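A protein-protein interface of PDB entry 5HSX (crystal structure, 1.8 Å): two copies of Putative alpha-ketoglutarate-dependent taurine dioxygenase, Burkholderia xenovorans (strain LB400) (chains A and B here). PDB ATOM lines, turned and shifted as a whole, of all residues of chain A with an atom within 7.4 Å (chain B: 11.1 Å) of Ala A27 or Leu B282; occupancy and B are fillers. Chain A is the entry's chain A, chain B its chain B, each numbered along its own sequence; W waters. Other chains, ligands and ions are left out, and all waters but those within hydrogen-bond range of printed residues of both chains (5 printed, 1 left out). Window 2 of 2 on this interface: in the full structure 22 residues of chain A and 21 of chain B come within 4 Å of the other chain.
No position is printed for both chains.
Hydrophobic or aromatic side chains of chain A within 4 Å of the printed part of chain B: Pro A24, Ala A27 and His A28.
Along chain A the printed residues that touch a printed residue of chain B span positions 24 to 253.
Of the 21 printed residues of chain B, 5 touch a printed residue of chain A.
Hydrophobic or aromatic side chains of chain B within 4 Å of the printed part of chain A: Tyr B146 and Leu B282.
Along chain B the printed residues that touch a printed residue of chain A span positions 146 to 282.
Among the printed residues, 6 pairs touch across the chains.
Water W1 lies within hydrogen-bond range of the side-chain carboxylate of Asp B149 (2.5 Å) and the backbone carbonyl oxygen of Leu A25 (2.8 Å).
Water W4 lies within hydrogen-bond range of the backbone carbonyl oxygen of Thr A253 (2.6 Å) and the guanidinium group of Arg B255 (3.1 Å).
Water W2 lies within hydrogen-bond range of OD1 of Asp B149, O of Leu A25 and N of Gly B147.
Water W5 bridges O of Pro A24 (2.7 Å) and O of Pro B145 (2.9 Å).
Water W3 lies within hydrogen-bond range of the side-chain amino group of Lys B257 (2.9 Å), the backbone carbonyl oxygen of Pro A24 (3.0 Å) and the backbone carbonyl oxygen of Pro B145 (3.2 Å).
Of the printed residues of chain B, Leu A25 touches Lys B257.
Printed residues of chain B within 4 Å of Ala A27: Leu B282 (3.999 Å).
Ile B143 touches none of the printed residues of chain A.
Pro B276 touches none of the printed residues of chain A.
Printed residues of chain A within 4 Å of Asp B281: His A28.
Printed residues of chain A within 4 Å of Leu B282: Ala A27.
The nearest printed residue of chain A that does not touch Leu B282 is His A28 (5.3 Å).
The nearest printed residue of chain B that does not touch Leu A25 is Tyr B146 (4.2 Å).
A ring nitrogen (NE2) of His A28 sits at hydrogen-bond distance from the side-chain carboxylate (OD1) of Asp B281.
O of Thr A253 lies within hydrogen-bond range of NH1 of Arg B255 (3.2 Å).
O of Pro B145 lies within hydrogen-bond range of NZ of Lys B257 (2.7 Å).
OD2 of Asp B149 lies within salt-bridge range of NE of Arg B255 (2.9 Å).
The backbone NH (N) of Leu A25 is in hydrogen-bond range of the backbone carbonyl oxygen (O) of Gly A30 (2.8 Å).
The backbone carbonyl oxygen (O) of His A28 sits at hydrogen-bond distance from the side-chain amide nitrogen (ND2) of Asn A154 (3.0 Å).
OG of Ser A26 is in hydrogen-bond range of O of Ile A29 (2.6 Å).
CB of Tyr B146 touches O of Pro A24 (3.6 Å).
Lys B257 touches Leu A25.
O of Ser A26 touches CD1 of Tyr B146 (3.2 Å).
Leu B282 touches Ala A27.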
ATOM      1  N   PRO A  24     -18.168  10.442 -19.115  1.00  0.00           N
ATOM      2  CA  PRO A  24     -19.553  10.037 -18.844  1.00  0.00           C
ATOM      3  C   PRO A  24     -20.344   9.884 -20.132  1.00  0.00           C
ATOM      4  O   PRO A  24     -20.066  10.537 -21.142  1.00  0.00           O
ATOM      5  CB  PRO A  24     -20.101  11.178 -17.978  1.00  0.00           C
ATOM      6  CG  PRO A  24     -18.856  11.843 -17.391  1.00  0.00           C
ATOM      7  CD  PRO A  24     -17.809  11.710 -18.452  1.00  0.00           C
ATOM      8  N   LEU A  25     -21.336   8.997 -20.089  1.00  0.00           N
ATOM      9  CA  LEU A  25     -22.133   8.691 -21.274  1.00  0.00           C
ATOM     10  C   LEU A  25     -23.580   9.149 -21.167  1.00  0.00           C
ATOM     11  O   LEU A  25     -24.288   9.160 -22.183  1.00  0.00           O
ATOM     12  CB  LEU A  25     -22.098   7.184 -21.557  1.00  0.00           C
ATOM     13  CG  LEU A  25     -20.715   6.642 -21.908  1.00  0.00           C
ATOM     14  CD1 LEU A  25     -20.735   5.127 -21.912  1.00  0.00           C
ATOM     15  CD2 LEU A  25     -20.288   7.177 -23.275  1.00  0.00           C
ATOM     16  N   SER A  26     -24.032   9.517 -19.979  1.00  0.00           N
ATOM     17  CA  SER A  26     -25.364  10.071 -19.772  1.00  0.00           C
ATOM     18  C   SER A  26     -25.318  10.910 -18.502  1.00  0.00           C
ATOM     19  O   SER A  26     -24.267  11.056 -17.873  1.00  0.00           O
ATOM     20  CB  SER A  26     -26.423   8.969 -19.684  1.00  0.00           C
ATOM     21  OG  SER A  26     -26.384   8.348 -18.412  1.00  0.00           O
ATOM     22  N   ALA A  27     -26.471  11.465 -18.122  1.00  0.00           N
ATOM     23  CA  ALA A  27     -26.486  12.399 -17.001  1.00  0.00           C
ATOM     24  C   ALA A  27     -26.043  11.728 -15.705  1.00  0.00           C
ATOM     25  O   ALA A  27     -25.301  12.324 -14.913  1.00  0.00           O
ATOM     26  CB  ALA A  27     -27.881  13.012 -16.849  1.00  0.00           C
ATOM     27  N   HIS A  28     -26.453  10.477 -15.474  1.00  0.00           N
ATOM     28  CA  HIS A  28     -26.149   9.852 -14.192  1.00  0.00           C
ATOM     29  C   HIS A  28     -25.769   8.375 -14.278  1.00  0.00           C
ATOM     30  O   HIS A  28     -25.683   7.720 -13.230  1.00  0.00           O
ATOM     31  CB  HIS A  28     -27.332  10.004 -13.222  1.00  0.00           C
ATOM     32  CG  HIS A  28     -27.712  11.426 -12.938  1.00  0.00           C
ATOM     33  ND1 HIS A  28     -26.979  12.238 -12.098  1.00  0.00           N
ATOM     34  CD2 HIS A  28     -28.756  12.171 -13.368  1.00  0.00           C
ATOM     35  CE1 HIS A  28     -27.550  13.430 -12.034  1.00  0.00           C
ATOM     36  NE2 HIS A  28     -28.627  13.416 -12.798  1.00  0.00           N
ATOM     37  N   ILE A  29     -25.536   7.813 -15.465  1.00  0.00           N
ATOM     38  CA  ILE A  29     -25.107   6.412 -15.494  1.00  0.00           C
ATOM     39  C   ILE A  29     -24.245   6.144 -16.724  1.00  0.00           C
ATOM     40  O   ILE A  29     -24.579   6.551 -17.844  1.00  0.00           O
ATOM     41  CB  ILE A  29     -26.298   5.425 -15.418  1.00  0.00           C
ATOM     42  CG1 ILE A  29     -25.777   3.975 -15.442  1.00  0.00           C
ATOM     43  CG2 ILE A  29     -27.315   5.683 -16.544  1.00  0.00           C
ATOM     44  CD1 ILE A  29     -26.792   2.917 -15.034  1.00  0.00           C
ATOM     45  N   GLY A  30     -23.133   5.438 -16.503  1.00  0.00           N
ATOM     46  CA  GLY A  30     -22.278   4.973 -17.580  1.00  0.00           C
ATOM     47  C   GLY A  30     -21.131   5.915 -17.870  1.00  0.00           C
ATOM     48  O   GLY A  30     -21.337   7.125 -18.014  1.00  0.00           O
ATOM     49  N   TRP A  57     -20.529   6.060 -11.353  1.00  0.00           N
ATOM     50  CA  TRP A  57     -21.255   5.999 -12.618  1.00  0.00           C
ATOM     51  C   TRP A  57     -22.011   4.692 -12.829  1.00  0.00           C
ATOM     52  O   TRP A  57     -22.696   4.549 -13.856  1.00  0.00           O
ATOM     53  CB  TRP A  57     -20.285   6.265 -13.776  1.00  0.00           C
ATOM     54  CG  TRP A  57     -19.847   7.703 -13.816  1.00  0.00           C
ATOM     55  CD1 TRP A  57     -18.627   8.212 -13.442  1.00  0.00           C
ATOM     56  CD2 TRP A  57     -20.650   8.828 -14.195  1.00  0.00           C
ATOM     57  NE1 TRP A  57     -18.622   9.580 -13.590  1.00  0.00           N
ATOM     58  CE2 TRP A  57     -19.849   9.984 -14.050  1.00  0.00           C
ATOM     59  CE3 TRP A  57     -21.963   8.970 -14.664  1.00  0.00           C
ATOM     60  CZ2 TRP A  57     -20.321  11.263 -14.354  1.00  0.00           C
ATOM     61  CZ3 TRP A  57     -22.434  10.242 -14.961  1.00  0.00           C
ATOM     62  CH2 TRP A  57     -21.613  11.371 -14.810  1.00  0.00           C
ATOM     63  N   ASN A 154     -30.133   2.864 -13.606  1.00  0.00           N
ATOM     64  CA  ASN A 154     -29.592   3.367 -12.346  1.00  0.00           C
ATOM     65  C   ASN A 154     -30.672   3.255 -11.275  1.00  0.00           C
ATOM     66  O   ASN A 154     -31.586   4.075 -11.218  1.00  0.00           O
ATOM     67  CB  ASN A 154     -29.124   4.809 -12.538  1.00  0.00           C
ATOM     68  CG  ASN A 154     -28.479   5.393 -11.292  1.00  0.00           C
ATOM     69  OD1 ASN A 154     -28.656   4.882 -10.187  1.00  0.00           O
ATOM     70  ND2 ASN A 154     -27.757   6.493 -11.467  1.00  0.00           N
ATOM     71  N   GLU A 251     -34.602   8.095 -18.840  1.00  0.00           N
ATOM     72  CA  GLU A 251     -33.719   8.980 -18.091  1.00  0.00           C
ATOM     73  C   GLU A 251     -32.818   8.232 -17.110  1.00  0.00           C
ATOM     74  O   GLU A 251     -31.825   8.803 -16.648  1.00  0.00           O
ATOM     75  CB  GLU A 251     -34.557  10.016 -17.336  1.00  0.00           C
ATOM     76  CG  GLU A 251     -35.827   9.436 -16.732  1.00  0.00           C
ATOM     77  CD  GLU A 251     -37.079   9.697 -17.583  1.00  0.00           C
ATOM     78  OE1 GLU A 251     -37.992  10.373 -17.059  1.00  0.00           O
ATOM     79  OE2 GLU A 251     -37.156   9.233 -18.759  1.00  0.00           O
ATOM     80  N   THR A 253     -31.361   5.228 -17.861  1.00  0.00           N
ATOM     81  CA  THR A 253     -30.666   4.155 -18.563  1.00  0.00           C
ATOM     82  C   THR A 253     -29.484   4.653 -19.390  1.00  0.00           C
ATOM     83  O   THR A 253     -29.358   5.840 -19.712  1.00  0.00           O
ATOM     84  CB  THR A 253     -31.616   3.388 -19.496  1.00  0.00           C
ATOM     85  OG1 THR A 253     -31.991   4.222 -20.593  1.00  0.00           O
ATOM     86  CG2 THR A 253     -32.867   2.955 -18.741  1.00  0.00           C
ATOM     87  N   SER B 102     -33.274  24.913 -28.728  1.00  0.00           N
ATOM     88  CA  SER B 102     -32.358  25.180 -27.627  1.00  0.00           C
ATOM     89  C   SER B 102     -33.035  25.001 -26.272  1.00  0.00           C
ATOM     90  O   SER B 102     -32.366  24.910 -25.242  1.00  0.00           O
ATOM     91  CB  SER B 102     -31.776  26.592 -27.745  1.00  0.00           C
ATOM     92  OG  SER B 102     -32.801  27.558 -27.878  1.00  0.00           O
ATOM     93  N   ILE B 143     -23.227  21.221 -28.478  1.00  0.00           N
ATOM     94  CA  ILE B 143     -23.676  19.921 -27.990  1.00  0.00           C
ATOM     95  C   ILE B 143     -22.979  19.603 -26.675  1.00  0.00           C
ATOM     96  O   ILE B 143     -21.743  19.663 -26.595  1.00  0.00           O
ATOM     97  CB  ILE B 143     -23.426  18.817 -29.028  1.00  0.00           C
ATOM     98  CG1 ILE B 143     -24.297  19.036 -30.276  1.00  0.00           C
ATOM     99  CG2 ILE B 143     -23.633  17.447 -28.405  1.00  0.00           C
ATOM    100  CD1 ILE B 143     -25.806  19.026 -30.016  1.00  0.00           C
ATOM    101  N   PRO B 144     -23.737  19.264 -25.631  1.00  0.00           N
ATOM    102  CA  PRO B 144     -23.119  18.973 -24.335  1.00  0.00           C
ATOM    103  C   PRO B 144     -22.228  17.747 -24.405  1.00  0.00           C
ATOM    104  O   PRO B 144     -22.482  16.820 -25.195  1.00  0.00           O
ATOM    105  CB  PRO B 144     -24.329  18.722 -23.418  1.00  0.00           C
ATOM    106  CG  PRO B 144     -25.472  19.446 -24.092  1.00  0.00           C
ATOM    107  CD  PRO B 144     -25.207  19.299 -25.566  1.00  0.00           C
ATOM    108  N   PRO B 145     -21.182  17.678 -23.570  1.00  0.00           N
ATOM    109  CA  PRO B 145     -20.337  16.467 -23.541  1.00  0.00           C
ATOM    110  C   PRO B 145     -21.105  15.195 -23.222  1.00  0.00           C
ATOM    111  O   PRO B 145     -20.701  14.113 -23.665  1.00  0.00           O
ATOM    112  CB  PRO B 145     -19.293  16.784 -22.455  1.00  0.00           C
ATOM    113  CG  PRO B 145     -19.854  17.918 -21.675  1.00  0.00           C
ATOM    114  CD  PRO B 145     -20.715  18.704 -22.624  1.00  0.00           C
ATOM    115  N   TYR B 146     -22.196  15.286 -22.467  1.00  0.00           N
ATOM    116  CA  TYR B 146     -23.060  14.134 -22.241  1.00  0.00           C
ATOM    117  C   TYR B 146     -24.433  14.639 -21.827  1.00  0.00           C
ATOM    118  O   TYR B 146     -24.609  15.809 -21.476  1.00  0.00           O
ATOM    119  CB  TYR B 146     -22.478  13.176 -21.195  1.00  0.00           C
ATOM    120  CG  TYR B 146     -22.158  13.827 -19.869  1.00  0.00           C
ATOM    121  CD1 TYR B 146     -23.085  13.832 -18.834  1.00  0.00           C
ATOM    122  CD2 TYR B 146     -20.930  14.441 -19.654  1.00  0.00           C
ATOM    123  CE1 TYR B 146     -22.789  14.427 -17.613  1.00  0.00           C
ATOM    124  CE2 TYR B 146     -20.632  15.036 -18.443  1.00  0.00           C
ATOM    125  CZ  TYR B 146     -21.569  15.029 -17.432  1.00  0.00           C
ATOM    126  OH  TYR B 146     -21.270  15.622 -16.229  1.00  0.00           O
ATOM    127  N   GLY B 147     -25.398  13.730 -21.854  1.00  0.00           N
ATOM    128  CA  GLY B 147     -26.794  14.089 -21.777  1.00  0.00           C
ATOM    129  C   GLY B 147     -27.336  14.488 -23.139  1.00  0.00           C
ATOM    130  O   GLY B 147     -26.600  14.843 -24.060  1.00  0.00           O
ATOM    131  N   GLY B 148     -28.653  14.406 -23.271  1.00  0.00           N
ATOM    132  CA  GLY B 148     -29.307  14.896 -24.466  1.00  0.00           C
ATOM    133  C   GLY B 148     -29.423  13.926 -25.621  1.00  0.00           C
ATOM    134  O   GLY B 148     -29.629  14.374 -26.755  1.00  0.00           O
ATOM    135  N   ASP B 149     -29.287  12.619 -25.383  1.00  0.00           N
ATOM    136  CA  ASP B 149     -29.412  11.644 -26.460  1.00  0.00           C
ATOM    137  C   ASP B 149     -30.832  11.645 -27.025  1.00  0.00           C
ATOM    138  O   ASP B 149     -31.799  11.940 -26.323  1.00  0.00           O
ATOM    139  CB  ASP B 149     -29.073  10.231 -25.965  1.00  0.00           C
ATOM    140  CG  ASP B 149     -27.604  10.051 -25.572  1.00  0.00           C
ATOM    141  OD1 ASP B 149     -26.797  11.011 -25.635  1.00  0.00           O
ATOM    142  OD2 ASP B 149     -27.272   8.919 -25.161  1.00  0.00           O
ATOM    143  N   ARG B 255     -30.593   4.512 -30.212  1.00  0.00           N
ATOM    144  CA  ARG B 255     -30.242   5.688 -29.425  1.00  0.00           C
ATOM    145  C   ARG B 255     -29.008   6.348 -30.028  1.00  0.00           C
ATOM    146  O   ARG B 255     -28.081   5.659 -30.471  1.00  0.00           O
ATOM    147  CB  ARG B 255     -29.991   5.286 -27.963  1.00  0.00           C
ATOM    148  CG  ARG B 255     -29.646   6.432 -27.013  1.00  0.00           C
ATOM    149  CD  ARG B 255     -29.716   5.924 -25.581  1.00  0.00           C
ATOM    150  NE  ARG B 255     -29.270   6.930 -24.629  1.00  0.00           N
ATOM    151  CZ  ARG B 255     -29.477   6.848 -23.317  1.00  0.00           C
ATOM    152  NH1 ARG B 255     -30.149   5.821 -22.820  1.00  0.00           N
ATOM    153  NH2 ARG B 255     -29.023   7.809 -22.506  1.00  0.00           N
ATOM    154  N   LYS B 257     -26.074   9.421 -29.478  1.00  0.00           N
ATOM    155  CA  LYS B 257     -25.403  10.404 -28.643  1.00  0.00           C
ATOM    156  C   LYS B 257     -24.796  11.461 -29.550  1.00  0.00           C
ATOM    157  O   LYS B 257     -23.933  11.154 -30.383  1.00  0.00           O
ATOM    158  CB  LYS B 257     -24.336   9.765 -27.754  1.00  0.00           C
ATOM    159  CG  LYS B 257     -23.613  10.802 -26.898  1.00  0.00           C
ATOM    160  CD  LYS B 257     -22.725  10.143 -25.859  1.00  0.00           C
ATOM    161  CE  LYS B 257     -22.152  11.175 -24.882  1.00  0.00           C
ATOM    162  NZ  LYS B 257     -21.262  12.188 -25.530  1.00  0.00           N
ATOM    163  N   PRO B 276     -34.714  14.249 -25.665  1.00  0.00           N
ATOM    164  CA  PRO B 276     -34.166  14.063 -24.324  1.00  0.00           C
ATOM    165  C   PRO B 276     -34.875  14.934 -23.303  1.00  0.00           C
ATOM    166  O   PRO B 276     -35.365  16.021 -23.612  1.00  0.00           O
ATOM    167  CB  PRO B 276     -32.703  14.486 -24.481  1.00  0.00           C
ATOM    168  CG  PRO B 276     -32.734  15.471 -25.597  1.00  0.00           C
ATOM    169  CD  PRO B 276     -33.751  14.913 -26.560  1.00  0.00           C
ATOM    170  N   THR B 277     -34.932  14.433 -22.075  1.00  0.00           N
ATOM    171  CA  THR B 277     -35.390  15.218 -20.943  1.00  0.00           C
ATOM    172  C   THR B 277     -34.288  15.484 -19.929  1.00  0.00           C
ATOM    173  O   THR B 277     -34.475  16.320 -19.039  1.00  0.00           O
ATOM    174  CB  THR B 277     -36.564  14.520 -20.242  1.00  0.00           C
ATOM    175  OG1 THR B 277     -36.141  13.242 -19.753  1.00  0.00           O
ATOM    176  CG2 THR B 277     -37.724  14.335 -21.209  1.00  0.00           C
ATOM    177  N   ASP B 278     -33.147  14.799 -20.046  1.00  0.00           N
ATOM    178  CA  ASP B 278     -32.042  14.955 -19.105  1.00  0.00           C
ATOM    179  C   ASP B 278     -31.272  16.257 -19.297  1.00  0.00           C
ATOM    180  O   ASP B 278     -30.373  16.541 -18.500  1.00  0.00           O
ATOM    181  CB  ASP B 278     -31.083  13.768 -19.231  1.00  0.00           C
ATOM    182  CG  ASP B 278     -30.469  13.648 -20.626  1.00  0.00           C
ATOM    183  OD1 ASP B 278     -30.892  14.384 -21.541  1.00  0.00           O
ATOM    184  OD2 ASP B 278     -29.570  12.805 -20.811  1.00  0.00           O
ATOM    185  N   ILE B 279     -31.580  17.039 -20.335  1.00  0.00           N
ATOM    186  CA  ILE B 279     -30.914  18.326 -20.506  1.00  0.00           C
ATOM    187  C   ILE B 279     -31.412  19.320 -19.462  1.00  0.00           C
ATOM    188  O   ILE B 279     -30.620  20.015 -18.817  1.00  0.00           O
ATOM    189  CB  ILE B 279     -31.100  18.853 -21.942  1.00  0.00           C
ATOM    190  CG1 ILE B 279     -32.577  18.858 -22.352  1.00  0.00           C
ATOM    191  CG2 ILE B 279     -30.288  18.022 -22.916  1.00  0.00           C
ATOM    192  CD1 ILE B 279     -32.815  19.324 -23.774  1.00  0.00           C
ATOM    193  N   PHE B 280     -32.732  19.387 -19.267  1.00  0.00           N
ATOM    194  CA  PHE B 280     -33.324  20.172 -18.186  1.00  0.00           C
ATOM    195  C   PHE B 280     -32.960  19.485 -16.872  1.00  0.00           C
ATOM    196  O   PHE B 280     -33.765  18.793 -16.244  1.00  0.00           O
ATOM    197  CB  PHE B 280     -34.833  20.295 -18.363  1.00  0.00           C
ATOM    198  N   ASP B 281     -31.709  19.696 -16.458  1.00  0.00           N
ATOM    199  CA  ASP B 281     -31.076  18.966 -15.367  1.00  0.00           C
ATOM    200  C   ASP B 281     -29.627  19.419 -15.256  1.00  0.00           C
ATOM    201  O   ASP B 281     -29.166  19.826 -14.185  1.00  0.00           O
ATOM    202  CB  ASP B 281     -31.138  17.455 -15.615  1.00  0.00           C
ATOM    203  CG  ASP B 281     -31.513  16.666 -14.378  1.00  0.00           C
ATOM    204  OD1 ASP B 281     -30.601  16.151 -13.696  1.00  0.00           O
ATOM    205  OD2 ASP B 281     -32.726  16.551 -14.098  1.00  0.00           O
ATOM    206  N   LEU B 282     -28.915  19.360 -16.377  1.00  0.00           N
ATOM    207  CA  LEU B 282     -27.492  19.645 -16.452  1.00  0.00           C
ATOM    208  C   LEU B 282     -27.245  21.095 -16.859  1.00  0.00           C
ATOM    209  O   LEU B 282     -28.115  21.775 -17.405  1.00  0.00           O
ATOM    210  CB  LEU B 282     -26.812  18.703 -17.446  1.00  0.00           C
ATOM    211  CG  LEU B 282     -26.907  17.197 -17.184  1.00  0.00           C
ATOM    212  CD1 LEU B 282     -26.474  16.409 -18.421  1.00  0.00           C
ATOM    213  CD2 LEU B 282     -26.070  16.806 -15.967  1.00  0.00           C
ATOM    214  N   ASP B 283     -26.020  21.552 -16.604  1.00  0.00           N
ATOM    215  CA  ASP B 283     -25.645  22.943 -16.816  1.00  0.00           C
ATOM    216  C   ASP B 283     -25.365  23.281 -18.275  1.00  0.00           C
ATOM    217  O   ASP B 283     -25.292  24.467 -18.613  1.00  0.00           O
ATOM    218  CB  ASP B 283     -24.408  23.270 -15.972  1.00  0.00           C
ATOM    219  CG  ASP B 283     -24.452  24.666 -15.385  1.00  0.00           C
ATOM    220  OD1 ASP B 283     -25.216  25.506 -15.903  1.00  0.00           O
ATOM    221  OD2 ASP B 283     -23.719  24.922 -14.406  1.00  0.00           O
ATOM    222  N   PHE B 284     -25.228  22.285 -19.144  1.00  0.00           N
ATOM    223  CA  PHE B 284     -24.662  22.500 -20.468  1.00  0.00           C
ATOM    224  C   PHE B 284     -25.645  23.186 -21.412  1.00  0.00           C
ATOM    225  O   PHE B 284     -26.847  22.907 -21.399  1.00  0.00           O
ATOM    226  CB  PHE B 284     -24.236  21.171 -21.087  1.00  0.00           C
ATOM    227  CG  PHE B 284     -23.332  20.343 -20.221  1.00  0.00           C
ATOM    228  CD1 PHE B 284     -23.694  19.052 -19.858  1.00  0.00           C
ATOM    229  CD2 PHE B 284     -22.116  20.842 -19.788  1.00  0.00           C
ATOM    230  CE1 PHE B 284     -22.862  18.275 -19.071  1.00  0.00           C
ATOM    231  CE2 PHE B 284     -21.276  20.074 -18.989  1.00  0.00           C
ATOM    232  CZ  PHE B 284     -21.651  18.789 -18.632  1.00  0.00           C
ATOM    233  N   ASP B 285     -25.115  24.060 -22.263  1.00  0.00           N
ATOM    234  CA  ASP B 285     -25.907  24.657 -23.324  1.00  0.00           C
ATOM    235  C   ASP B 285     -26.065  23.669 -24.473  1.00  0.00           C
ATOM    236  O   ASP B 285     -25.220  22.797 -24.690  1.00  0.00           O
ATOM    237  CB  ASP B 285     -25.259  25.948 -23.822  1.00  0.00           C
ATOM    238  CG  ASP B 285     -25.460  27.105 -22.865  1.00  0.00           C
ATOM    239  OD1 ASP B 285     -25.674  26.854 -21.661  1.00  0.00           O
ATOM    240  OD2 ASP B 285     -25.405  28.268 -23.319  1.00  0.00           O
ATOM    241  N   ARG B 286     -27.163  23.812 -25.212  1.00  0.00           N
ATOM    242  CA  ARG B 286     -27.486  22.877 -26.284  1.00  0.00           C
ATOM    243  C   ARG B 286     -28.215  23.640 -27.378  1.00  0.00           C
ATOM    244  O   ARG B 286     -29.280  24.211 -27.125  1.00  0.00           O
ATOM    245  CB  ARG B 286     -28.341  21.722 -25.757  1.00  0.00           C
ATOM    246  CG  ARG B 286     -28.586  20.584 -26.740  1.00  0.00           C
ATOM    247  CD  ARG B 286     -29.303  19.439 -26.035  1.00  0.00           C
ATOM    248  NE  ARG B 286     -29.490  18.242 -26.853  1.00  0.00           N
ATOM    249  CZ  ARG B 286     -30.598  17.980 -27.542  1.00  0.00           C
ATOM    250  NH1 ARG B 286     -31.607  18.843 -27.521  1.00  0.00           N
ATOM    251  NH2 ARG B 286     -30.702  16.863 -28.251  1.00  0.00           N
HETATM  252  O   HOH W   1     -25.181   7.757 -24.384  1.00  0.00           O
HETATM  253  O   HOH W   2     -25.556  11.322 -23.324  1.00  0.00           O
HETATM  254  O   HOH W   3     -19.052  11.351 -23.899  1.00  0.00           O
HETATM  255  O   HOH W   4     -30.143   8.360 -19.697  1.00  0.00           O
HETATM  256  O   HOH W   5     -18.833  12.795 -21.931  1.00  0.00           O
